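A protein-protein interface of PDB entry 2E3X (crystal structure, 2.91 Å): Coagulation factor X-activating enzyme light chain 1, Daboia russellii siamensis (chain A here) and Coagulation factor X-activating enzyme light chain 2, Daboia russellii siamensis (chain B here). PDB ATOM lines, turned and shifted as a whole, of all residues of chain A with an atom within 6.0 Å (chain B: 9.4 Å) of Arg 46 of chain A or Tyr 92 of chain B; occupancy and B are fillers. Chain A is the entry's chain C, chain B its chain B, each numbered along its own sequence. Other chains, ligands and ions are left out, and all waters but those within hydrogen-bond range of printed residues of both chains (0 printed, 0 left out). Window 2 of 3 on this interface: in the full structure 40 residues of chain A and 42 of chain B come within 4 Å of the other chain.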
ATOM      1  N   LEU A  43     -25.815  11.146 -22.818  1.00  0.00           N
ATOM      2  CA  LEU A  43     -27.268  11.100 -22.729  1.00  0.00           C
ATOM      3  C   LEU A  43     -27.909  11.043 -24.106  1.00  0.00           C
ATOM      4  O   LEU A  43     -27.880  12.019 -24.857  1.00  0.00           O
ATOM      5  CB  LEU A  43     -27.784  12.324 -21.965  1.00  0.00           C
ATOM      6  CG  LEU A  43     -27.096  12.657 -20.635  1.00  0.00           C
ATOM      7  CD1 LEU A  43     -27.768  13.865 -20.013  1.00  0.00           C
ATOM      8  CD2 LEU A  43     -27.162  11.472 -19.689  1.00  0.00           C
ATOM      9  N   HIS A  44     -28.501   9.895 -24.427  1.00  0.00           N
ATOM     10  CA  HIS A  44     -29.142   9.700 -25.723  1.00  0.00           C
ATOM     11  C   HIS A  44     -30.665   9.687 -25.662  1.00  0.00           C
ATOM     12  O   HIS A  44     -31.323   9.300 -26.627  1.00  0.00           O
ATOM     13  CB  HIS A  44     -28.643   8.404 -26.350  1.00  0.00           C
ATOM     14  CG  HIS A  44     -27.160   8.362 -26.526  1.00  0.00           C
ATOM     15  ND1 HIS A  44     -26.493   9.190 -27.403  1.00  0.00           N
ATOM     16  CD2 HIS A  44     -26.209   7.617 -25.914  1.00  0.00           C
ATOM     17  CE1 HIS A  44     -25.196   8.957 -27.323  1.00  0.00           C
ATOM     18  NE2 HIS A  44     -24.997   8.008 -26.426  1.00  0.00           N
ATOM     19  N   SER A  45     -31.220  10.117 -24.531  1.00  0.00           N
ATOM     20  CA  SER A  45     -32.669  10.163 -24.353  1.00  0.00           C
ATOM     21  C   SER A  45     -33.059  10.717 -22.990  1.00  0.00           C
ATOM     22  O   SER A  45     -32.391  10.453 -21.988  1.00  0.00           O
ATOM     23  CB  SER A  45     -33.270   8.771 -24.509  1.00  0.00           C
ATOM     24  OG  SER A  45     -34.674   8.827 -24.336  1.00  0.00           O
ATOM     25  N   ARG A  46     -34.152  11.476 -22.956  1.00  0.00           N
ATOM     26  CA  ARG A  46     -34.624  12.061 -21.708  1.00  0.00           C
ATOM     27  C   ARG A  46     -34.719  10.990 -20.632  1.00  0.00           C
ATOM     28  O   ARG A  46     -34.523  11.257 -19.448  1.00  0.00           O
ATOM     29  CB  ARG A  46     -35.995  12.707 -21.898  1.00  0.00           C
ATOM     30  CG  ARG A  46     -36.556  13.311 -20.617  1.00  0.00           C
ATOM     31  CD  ARG A  46     -37.918  13.949 -20.838  1.00  0.00           C
ATOM     32  NE  ARG A  46     -38.464  14.501 -19.601  1.00  0.00           N
ATOM     33  CZ  ARG A  46     -39.628  15.138 -19.513  1.00  0.00           C
ATOM     34  NH1 ARG A  46     -40.379  15.307 -20.593  1.00  0.00           N
ATOM     35  NH2 ARG A  46     -40.042  15.608 -18.343  1.00  0.00           N
ATOM     36  N   GLU A  47     -35.019   9.770 -21.060  1.00  0.00           N
ATOM     37  CA  GLU A  47     -35.147   8.648 -20.145  1.00  0.00           C
ATOM     38  C   GLU A  47     -33.845   8.463 -19.384  1.00  0.00           C
ATOM     39  O   GLU A  47     -33.822   8.534 -18.159  1.00  0.00           O
ATOM     40  CB  GLU A  47     -35.486   7.375 -20.922  1.00  0.00           C
ATOM     41  CG  GLU A  47     -36.358   7.609 -22.155  1.00  0.00           C
ATOM     42  CD  GLU A  47     -37.645   8.366 -21.855  1.00  0.00           C
ATOM     43  OE1 GLU A  47     -38.374   8.700 -22.817  1.00  0.00           O
ATOM     44  OE2 GLU A  47     -37.930   8.625 -20.665  1.00  0.00           O
ATOM     45  N   GLU A  48     -32.758   8.229 -20.113  1.00  0.00           N
ATOM     46  CA  GLU A  48     -31.461   8.041 -19.477  1.00  0.00           C
ATOM     47  C   GLU A  48     -31.124   9.275 -18.659  1.00  0.00           C
ATOM     48  O   GLU A  48     -30.575   9.181 -17.559  1.00  0.00           O
ATOM     49  CB  GLU A  48     -30.365   7.816 -20.522  1.00  0.00           C
ATOM     50  CG  GLU A  48     -28.983   7.638 -19.906  1.00  0.00           C
ATOM     51  CD  GLU A  48     -27.880   7.489 -20.939  1.00  0.00           C
ATOM     52  OE1 GLU A  48     -26.719   7.274 -20.533  1.00  0.00           O
ATOM     53  OE2 GLU A  48     -28.169   7.589 -22.151  1.00  0.00           O
ATOM     54  N   GLU A  49     -31.460  10.436 -19.208  1.00  0.00           N
ATOM     55  CA  GLU A  49     -31.189  11.690 -18.532  1.00  0.00           C
ATOM     56  C   GLU A  49     -31.819  11.707 -17.143  1.00  0.00           C
ATOM     57  O   GLU A  49     -31.115  11.782 -16.136  1.00  0.00           O
ATOM     58  CB  GLU A  49     -31.711  12.859 -19.371  1.00  0.00           C
ATOM     59  CG  GLU A  49     -31.517  14.212 -18.717  1.00  0.00           C
ATOM     60  CD  GLU A  49     -31.798  15.358 -19.659  1.00  0.00           C
ATOM     61  OE1 GLU A  49     -32.909  15.408 -20.231  1.00  0.00           O
ATOM     62  OE2 GLU A  49     -30.901  16.212 -19.822  1.00  0.00           O
ATOM     63  N   LYS A  50     -33.144  11.624 -17.088  1.00  0.00           N
ATOM     64  CA  LYS A  50     -33.846  11.636 -15.813  1.00  0.00           C
ATOM     65  C   LYS A  50     -33.279  10.609 -14.836  1.00  0.00           C
ATOM     66  O   LYS A  50     -33.412  10.762 -13.623  1.00  0.00           O
ATOM     67  CB  LYS A  50     -35.343  11.396 -16.023  1.00  0.00           C
ATOM     68  CG  LYS A  50     -36.014  12.480 -16.855  1.00  0.00           C
ATOM     69  CD  LYS A  50     -37.534  12.453 -16.738  1.00  0.00           C
ATOM     70  CE  LYS A  50     -38.138  11.170 -17.287  1.00  0.00           C
ATOM     71  NZ  LYS A  50     -37.798   9.979 -16.460  1.00  0.00           N
ATOM     72  N   PHE A  51     -32.644   9.566 -15.360  1.00  0.00           N
ATOM     73  CA  PHE A  51     -32.052   8.553 -14.499  1.00  0.00           C
ATOM     74  C   PHE A  51     -30.809   9.129 -13.833  1.00  0.00           C
ATOM     75  O   PHE A  51     -30.623   9.008 -12.621  1.00  0.00           O
ATOM     76  CB  PHE A  51     -31.649   7.315 -15.300  1.00  0.00           C
ATOM     77  CG  PHE A  51     -30.781   6.362 -14.527  1.00  0.00           C
ATOM     78  CD1 PHE A  51     -31.304   5.626 -13.469  1.00  0.00           C
ATOM     79  CD2 PHE A  51     -29.426   6.238 -14.825  1.00  0.00           C
ATOM     80  CE1 PHE A  51     -30.489   4.780 -12.715  1.00  0.00           C
ATOM     81  CE2 PHE A  51     -28.604   5.396 -14.076  1.00  0.00           C
ATOM     82  CZ  PHE A  51     -29.137   4.667 -13.019  1.00  0.00           C
ATOM     83  N   LYS A 105     -33.233  20.463 -14.895  1.00  0.00           N
ATOM     84  CA  LYS A 105     -32.825  19.358 -15.756  1.00  0.00           C
ATOM     85  C   LYS A 105     -32.623  19.716 -17.227  1.00  0.00           C
ATOM     86  O   LYS A 105     -33.173  19.066 -18.116  1.00  0.00           O
ATOM     87  CB  LYS A 105     -33.816  18.192 -15.629  1.00  0.00           C
ATOM     88  CG  LYS A 105     -35.272  18.565 -15.840  1.00  0.00           C
ATOM     89  CD  LYS A 105     -36.195  17.391 -15.544  1.00  0.00           C
ATOM     90  CE  LYS A 105     -37.657  17.802 -15.644  1.00  0.00           C
ATOM     91  NZ  LYS A 105     -38.577  16.667 -15.355  1.00  0.00           N
ATOM     92  N   TRP A 107     -29.533  21.732 -20.153  1.00  0.00           N
ATOM     93  CA  TRP A 107     -28.103  21.854 -20.402  1.00  0.00           C
ATOM     94  C   TRP A 107     -27.641  23.302 -20.503  1.00  0.00           C
ATOM     95  O   TRP A 107     -28.312  24.149 -21.099  1.00  0.00           O
ATOM     96  CB  TRP A 107     -27.726  21.113 -21.683  1.00  0.00           C
ATOM     97  CG  TRP A 107     -27.930  19.632 -21.618  1.00  0.00           C
ATOM     98  CD1 TRP A 107     -28.361  18.906 -20.546  1.00  0.00           C
ATOM     99  CD2 TRP A 107     -27.697  18.692 -22.672  1.00  0.00           C
ATOM    100  NE1 TRP A 107     -28.410  17.570 -20.866  1.00  0.00           N
ATOM    101  CE2 TRP A 107     -28.007  17.412 -22.166  1.00  0.00           C
ATOM    102  CE3 TRP A 107     -27.255  18.807 -23.997  1.00  0.00           C
ATOM    103  CZ2 TRP A 107     -27.890  16.253 -22.939  1.00  0.00           C
ATOM    104  CZ3 TRP A 107     -27.140  17.654 -24.767  1.00  0.00           C
ATOM    105  CH2 TRP A 107     -27.456  16.395 -24.233  1.00  0.00           C
ATOM    106  N   GLN B  78     -25.733  22.141 -34.187  1.00  0.00           N
ATOM    107  CA  GLN B  78     -25.363  22.875 -32.985  1.00  0.00           C
ATOM    108  C   GLN B  78     -23.979  22.438 -32.512  1.00  0.00           C
ATOM    109  O   GLN B  78     -23.092  23.264 -32.297  1.00  0.00           O
ATOM    110  CB  GLN B  78     -26.409  22.620 -31.895  1.00  0.00           C
ATOM    111  CG  GLN B  78     -26.036  23.073 -30.490  1.00  0.00           C
ATOM    112  CD  GLN B  78     -25.078  22.122 -29.784  1.00  0.00           C
ATOM    113  OE1 GLN B  78     -23.859  22.269 -29.868  1.00  0.00           O
ATOM    114  NE2 GLN B  78     -25.632  21.133 -29.090  1.00  0.00           N
ATOM    115  N   GLU B  79     -23.805  21.129 -32.359  1.00  0.00           N
ATOM    116  CA  GLU B  79     -22.547  20.548 -31.902  1.00  0.00           C
ATOM    117  C   GLU B  79     -21.501  20.520 -33.010  1.00  0.00           C
ATOM    118  O   GLU B  79     -20.350  20.137 -32.782  1.00  0.00           O
ATOM    119  CB  GLU B  79     -22.784  19.121 -31.392  1.00  0.00           C
ATOM    120  CG  GLU B  79     -23.295  18.145 -32.456  1.00  0.00           C
ATOM    121  CD  GLU B  79     -24.743  18.394 -32.860  1.00  0.00           C
ATOM    122  OE1 GLU B  79     -25.179  17.829 -33.886  1.00  0.00           O
ATOM    123  OE2 GLU B  79     -25.449  19.142 -32.152  1.00  0.00           O
ATOM    124  N   TRP B  84     -19.921  12.845 -28.168  1.00  0.00           N
ATOM    125  CA  TRP B  84     -19.654  12.546 -26.772  1.00  0.00           C
ATOM    126  C   TRP B  84     -18.246  11.989 -26.598  1.00  0.00           C
ATOM    127  O   TRP B  84     -17.725  11.309 -27.481  1.00  0.00           O
ATOM    128  CB  TRP B  84     -20.699  11.564 -26.242  1.00  0.00           C
ATOM    129  CG  TRP B  84     -22.090  12.113 -26.331  1.00  0.00           C
ATOM    130  CD1 TRP B  84     -22.973  11.955 -27.362  1.00  0.00           C
ATOM    131  CD2 TRP B  84     -22.731  12.972 -25.382  1.00  0.00           C
ATOM    132  NE1 TRP B  84     -24.125  12.664 -27.113  1.00  0.00           N
ATOM    133  CE2 TRP B  84     -24.002  13.300 -25.906  1.00  0.00           C
ATOM    134  CE3 TRP B  84     -22.352  13.502 -24.140  1.00  0.00           C
ATOM    135  CZ2 TRP B  84     -24.900  14.133 -25.229  1.00  0.00           C
ATOM    136  CZ3 TRP B  84     -23.245  14.331 -23.468  1.00  0.00           C
ATOM    137  CH2 TRP B  84     -24.505  14.639 -24.016  1.00  0.00           C
ATOM    138  N   SER B  88     -19.842   7.843 -28.926  1.00  0.00           N
ATOM    139  CA  SER B  88     -21.187   7.812 -29.484  1.00  0.00           C
ATOM    140  C   SER B  88     -21.559   9.151 -30.103  1.00  0.00           C
ATOM    141  O   SER B  88     -21.128  10.204 -29.638  1.00  0.00           O
ATOM    142  CB  SER B  88     -22.210   7.437 -28.404  1.00  0.00           C
ATOM    143  OG  SER B  88     -22.226   8.383 -27.351  1.00  0.00           O
ATOM    144  N   SER B  89     -22.352   9.104 -31.164  1.00  0.00           N
ATOM    145  CA  SER B  89     -22.784  10.320 -31.838  1.00  0.00           C
ATOM    146  C   SER B  89     -23.743  11.051 -30.915  1.00  0.00           C
ATOM    147  O   SER B  89     -24.130  10.517 -29.878  1.00  0.00           O
ATOM    148  CB  SER B  89     -23.476   9.973 -33.159  1.00  0.00           C
ATOM    149  OG  SER B  89     -24.493   9.006 -32.960  1.00  0.00           O
ATOM    150  N   VAL B  90     -24.122  12.270 -31.283  1.00  0.00           N
ATOM    151  CA  VAL B  90     -25.032  13.049 -30.456  1.00  0.00           C
ATOM    152  C   VAL B  90     -26.482  12.828 -30.847  1.00  0.00           C
ATOM    153  O   VAL B  90     -27.054  13.577 -31.638  1.00  0.00           O
ATOM    154  CB  VAL B  90     -24.709  14.555 -30.519  1.00  0.00           C
ATOM    155  CG1 VAL B  90     -25.744  15.349 -29.737  1.00  0.00           C
ATOM    156  CG2 VAL B  90     -23.329  14.805 -29.938  1.00  0.00           C
ATOM    157  N   SER B  91     -27.068  11.784 -30.275  1.00  0.00           N
ATOM    158  CA  SER B  91     -28.457  11.433 -30.526  1.00  0.00           C
ATOM    159  C   SER B  91     -29.366  12.485 -29.890  1.00  0.00           C
ATOM    160  O   SER B  91     -29.946  13.326 -30.576  1.00  0.00           O
ATOM    161  CB  SER B  91     -28.745  10.052 -29.924  1.00  0.00           C
ATOM    162  OG  SER B  91     -30.103   9.677 -30.084  1.00  0.00           O
ATOM    163  N   TYR B  92     -29.471  12.430 -28.568  1.00  0.00           N
ATOM    164  CA  TYR B  92     -30.305  13.351 -27.806  1.00  0.00           C
ATOM    165  C   TYR B  92     -29.570  14.670 -27.592  1.00  0.00           C
ATOM    166  O   TYR B  92     -28.418  14.678 -27.158  1.00  0.00           O
ATOM    167  CB  TYR B  92     -30.656  12.709 -26.456  1.00  0.00           C
ATOM    168  CG  TYR B  92     -31.548  13.534 -25.552  1.00  0.00           C
ATOM    169  CD1 TYR B  92     -32.796  13.974 -25.984  1.00  0.00           C
ATOM    170  CD2 TYR B  92     -31.149  13.859 -24.254  1.00  0.00           C
ATOM    171  CE1 TYR B  92     -33.627  14.716 -25.147  1.00  0.00           C
ATOM    172  CE2 TYR B  92     -31.974  14.602 -23.411  1.00  0.00           C
ATOM    173  CZ  TYR B  92     -33.211  15.026 -23.867  1.00  0.00           C
ATOM    174  OH  TYR B  92     -34.035  15.764 -23.048  1.00  0.00           O
ATOM    175  N   ASP B  93     -30.236  15.780 -27.904  1.00  0.00           N
ATOM    176  CA  ASP B  93     -29.647  17.107 -27.727  1.00  0.00           C
ATOM    177  C   ASP B  93     -30.622  18.046 -27.045  1.00  0.00           C
ATOM    178  O   ASP B  93     -31.648  18.398 -27.622  1.00  0.00           O
ATOM    179  CB  ASP B  93     -29.260  17.721 -29.072  1.00  0.00           C
ATOM    180  CG  ASP B  93     -28.824  19.174 -28.944  1.00  0.00           C
ATOM    181  OD1 ASP B  93     -27.762  19.422 -28.335  1.00  0.00           O
ATOM    182  OD2 ASP B  93     -29.542  20.070 -29.442  1.00  0.00           O
ATOM    183  N   LYS B  94     -30.306  18.465 -25.824  1.00  0.00           N
ATOM    184  CA  LYS B  94     -31.196  19.373 -25.119  1.00  0.00           C
ATOM    185  C   LYS B  94     -30.502  20.638 -24.620  1.00  0.00           C
ATOM    186  O   LYS B  94     -30.777  21.124 -23.519  1.00  0.00           O
ATOM    187  CB  LYS B  94     -31.870  18.659 -23.948  1.00  0.00           C
ATOM    188  CG  LYS B  94     -30.976  18.436 -22.749  1.00  0.00           C
ATOM    189  CD  LYS B  94     -31.802  18.200 -21.500  1.00  0.00           C
ATOM    190  CE  LYS B  94     -32.656  19.410 -21.156  1.00  0.00           C
ATOM    191  NZ  LYS B  94     -33.678  19.738 -22.188  1.00  0.00           N
ATOM    192  N   LEU B  95     -29.598  21.169 -25.434  1.00  0.00           N
ATOM    193  CA  LEU B  95     -28.893  22.391 -25.080  1.00  0.00           C
ATOM    194  C   LEU B  95     -29.735  23.569 -25.566  1.00  0.00           C
ATOM    195  O   LEU B  95     -29.899  23.765 -26.770  1.00  0.00           O
ATOM    196  CB  LEU B  95     -27.524  22.437 -25.760  1.00  0.00           C
ATOM    197  CG  LEU B  95     -26.657  23.651 -25.411  1.00  0.00           C
ATOM    198  CD1 LEU B  95     -26.071  23.462 -24.021  1.00  0.00           C
ATOM    199  CD2 LEU B  95     -25.544  23.808 -26.421  1.00  0.00           C
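Among the printed residues, pairs that only touch across the chains: Glu 49 of chain A with Lys 94 of chain B, Lys 105 of chain A with Lys 94 of chain B, His 44 of chain A with Tyr 92 of chain B, His 44 of chain A with Ser 89 of chain B, Trp 107 of chain A with Lys 94 of chain B, Leu 43 of chain A with Tyr 92 of chain B, Ser 45 of chain A with Tyr 92 of chain B, Trp 107 of chain A with Trp 84 of chain B, His 44 of chain A with Ser 91 of chain B, Trp 107 of chain A with Tyr 92 of chain B, Trp 107 of chain A with Leu 95 of chain B, Leu 43 of chain A with Trp 84 of chain B, His 44 of chain A with Trp 84 of chain B, Arg 46 of chain A with Tyr 92 of chain B and Trp 107 of chain A with Asp 93 of chain B.
Of the 11 printed residues of chain A, 7 touch a printed residue of chain B. Hydrophobic or aromatic side chains of chain A within 4 Å of the printed part of chain B: His 44 and Trp 107. Hydrophobic or aromatic side chains of chain B that line the printed part of chain A: Trp 84, Tyr 92 and Leu 95. Along chain B the printed residues that touch a printed residue of chain A span positions 84 to 95. Among the printed residues, no Asp or Glu carboxylate lies within 4 Å of a Lys or Arg side-chain nitrogen of the other chain.
OD1 of Asp 93 of chain B is in hydrogen-bond range of NE2 of Gln 78 of chain B, 2.8 Å away. N of His 44 of chain A sits at hydrogen-bond distance from OE2 of Glu 48 of chain A. OG of Ser 45 of chain A lies close to N of Glu 47 of chain A (3.4 Å). The side-chain carboxylate of Glu 49 of chain A is in hydrogen-bond range of the indole nitrogen of Trp 107 of chain A.
OG of Ser 88 of chain B is in hydrogen-bond range of NE2 of His 44 of chain A, 2.9 Å away. The side-chain hydroxyl of Tyr 92 of chain B sits at hydrogen-bond distance from the side-chain carboxylate of Glu 49 of chain A, at 3.1 Å.
Of the printed residues of chain B, Leu 43 of chain A touches Trp 84 and Tyr 92. No residue of chain B comes within 4 Å of Glu 47 of chain A. Of chain B, only Tyr 92 (3.1 Å) and Lys 94 (2.8 Å) come within 4 Å of Glu 49 of chain A. Phe 51 of chain A touches none of the printed residues of chain B. Of the printed residues of chain B, Trp 107 of chain A touches Trp 84, Tyr 92, Asp 93, Lys 94 and Leu 95. Printed residues of chain A within 4 Å of Ser 91 of chain B: His 44. Of the printed residues of chain A, Leu 95 of chain B touches Trp 107. The nearest residue of chain B that does not touch Arg 46 of chain A is Lys 94 of chain B (6.8 Å).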
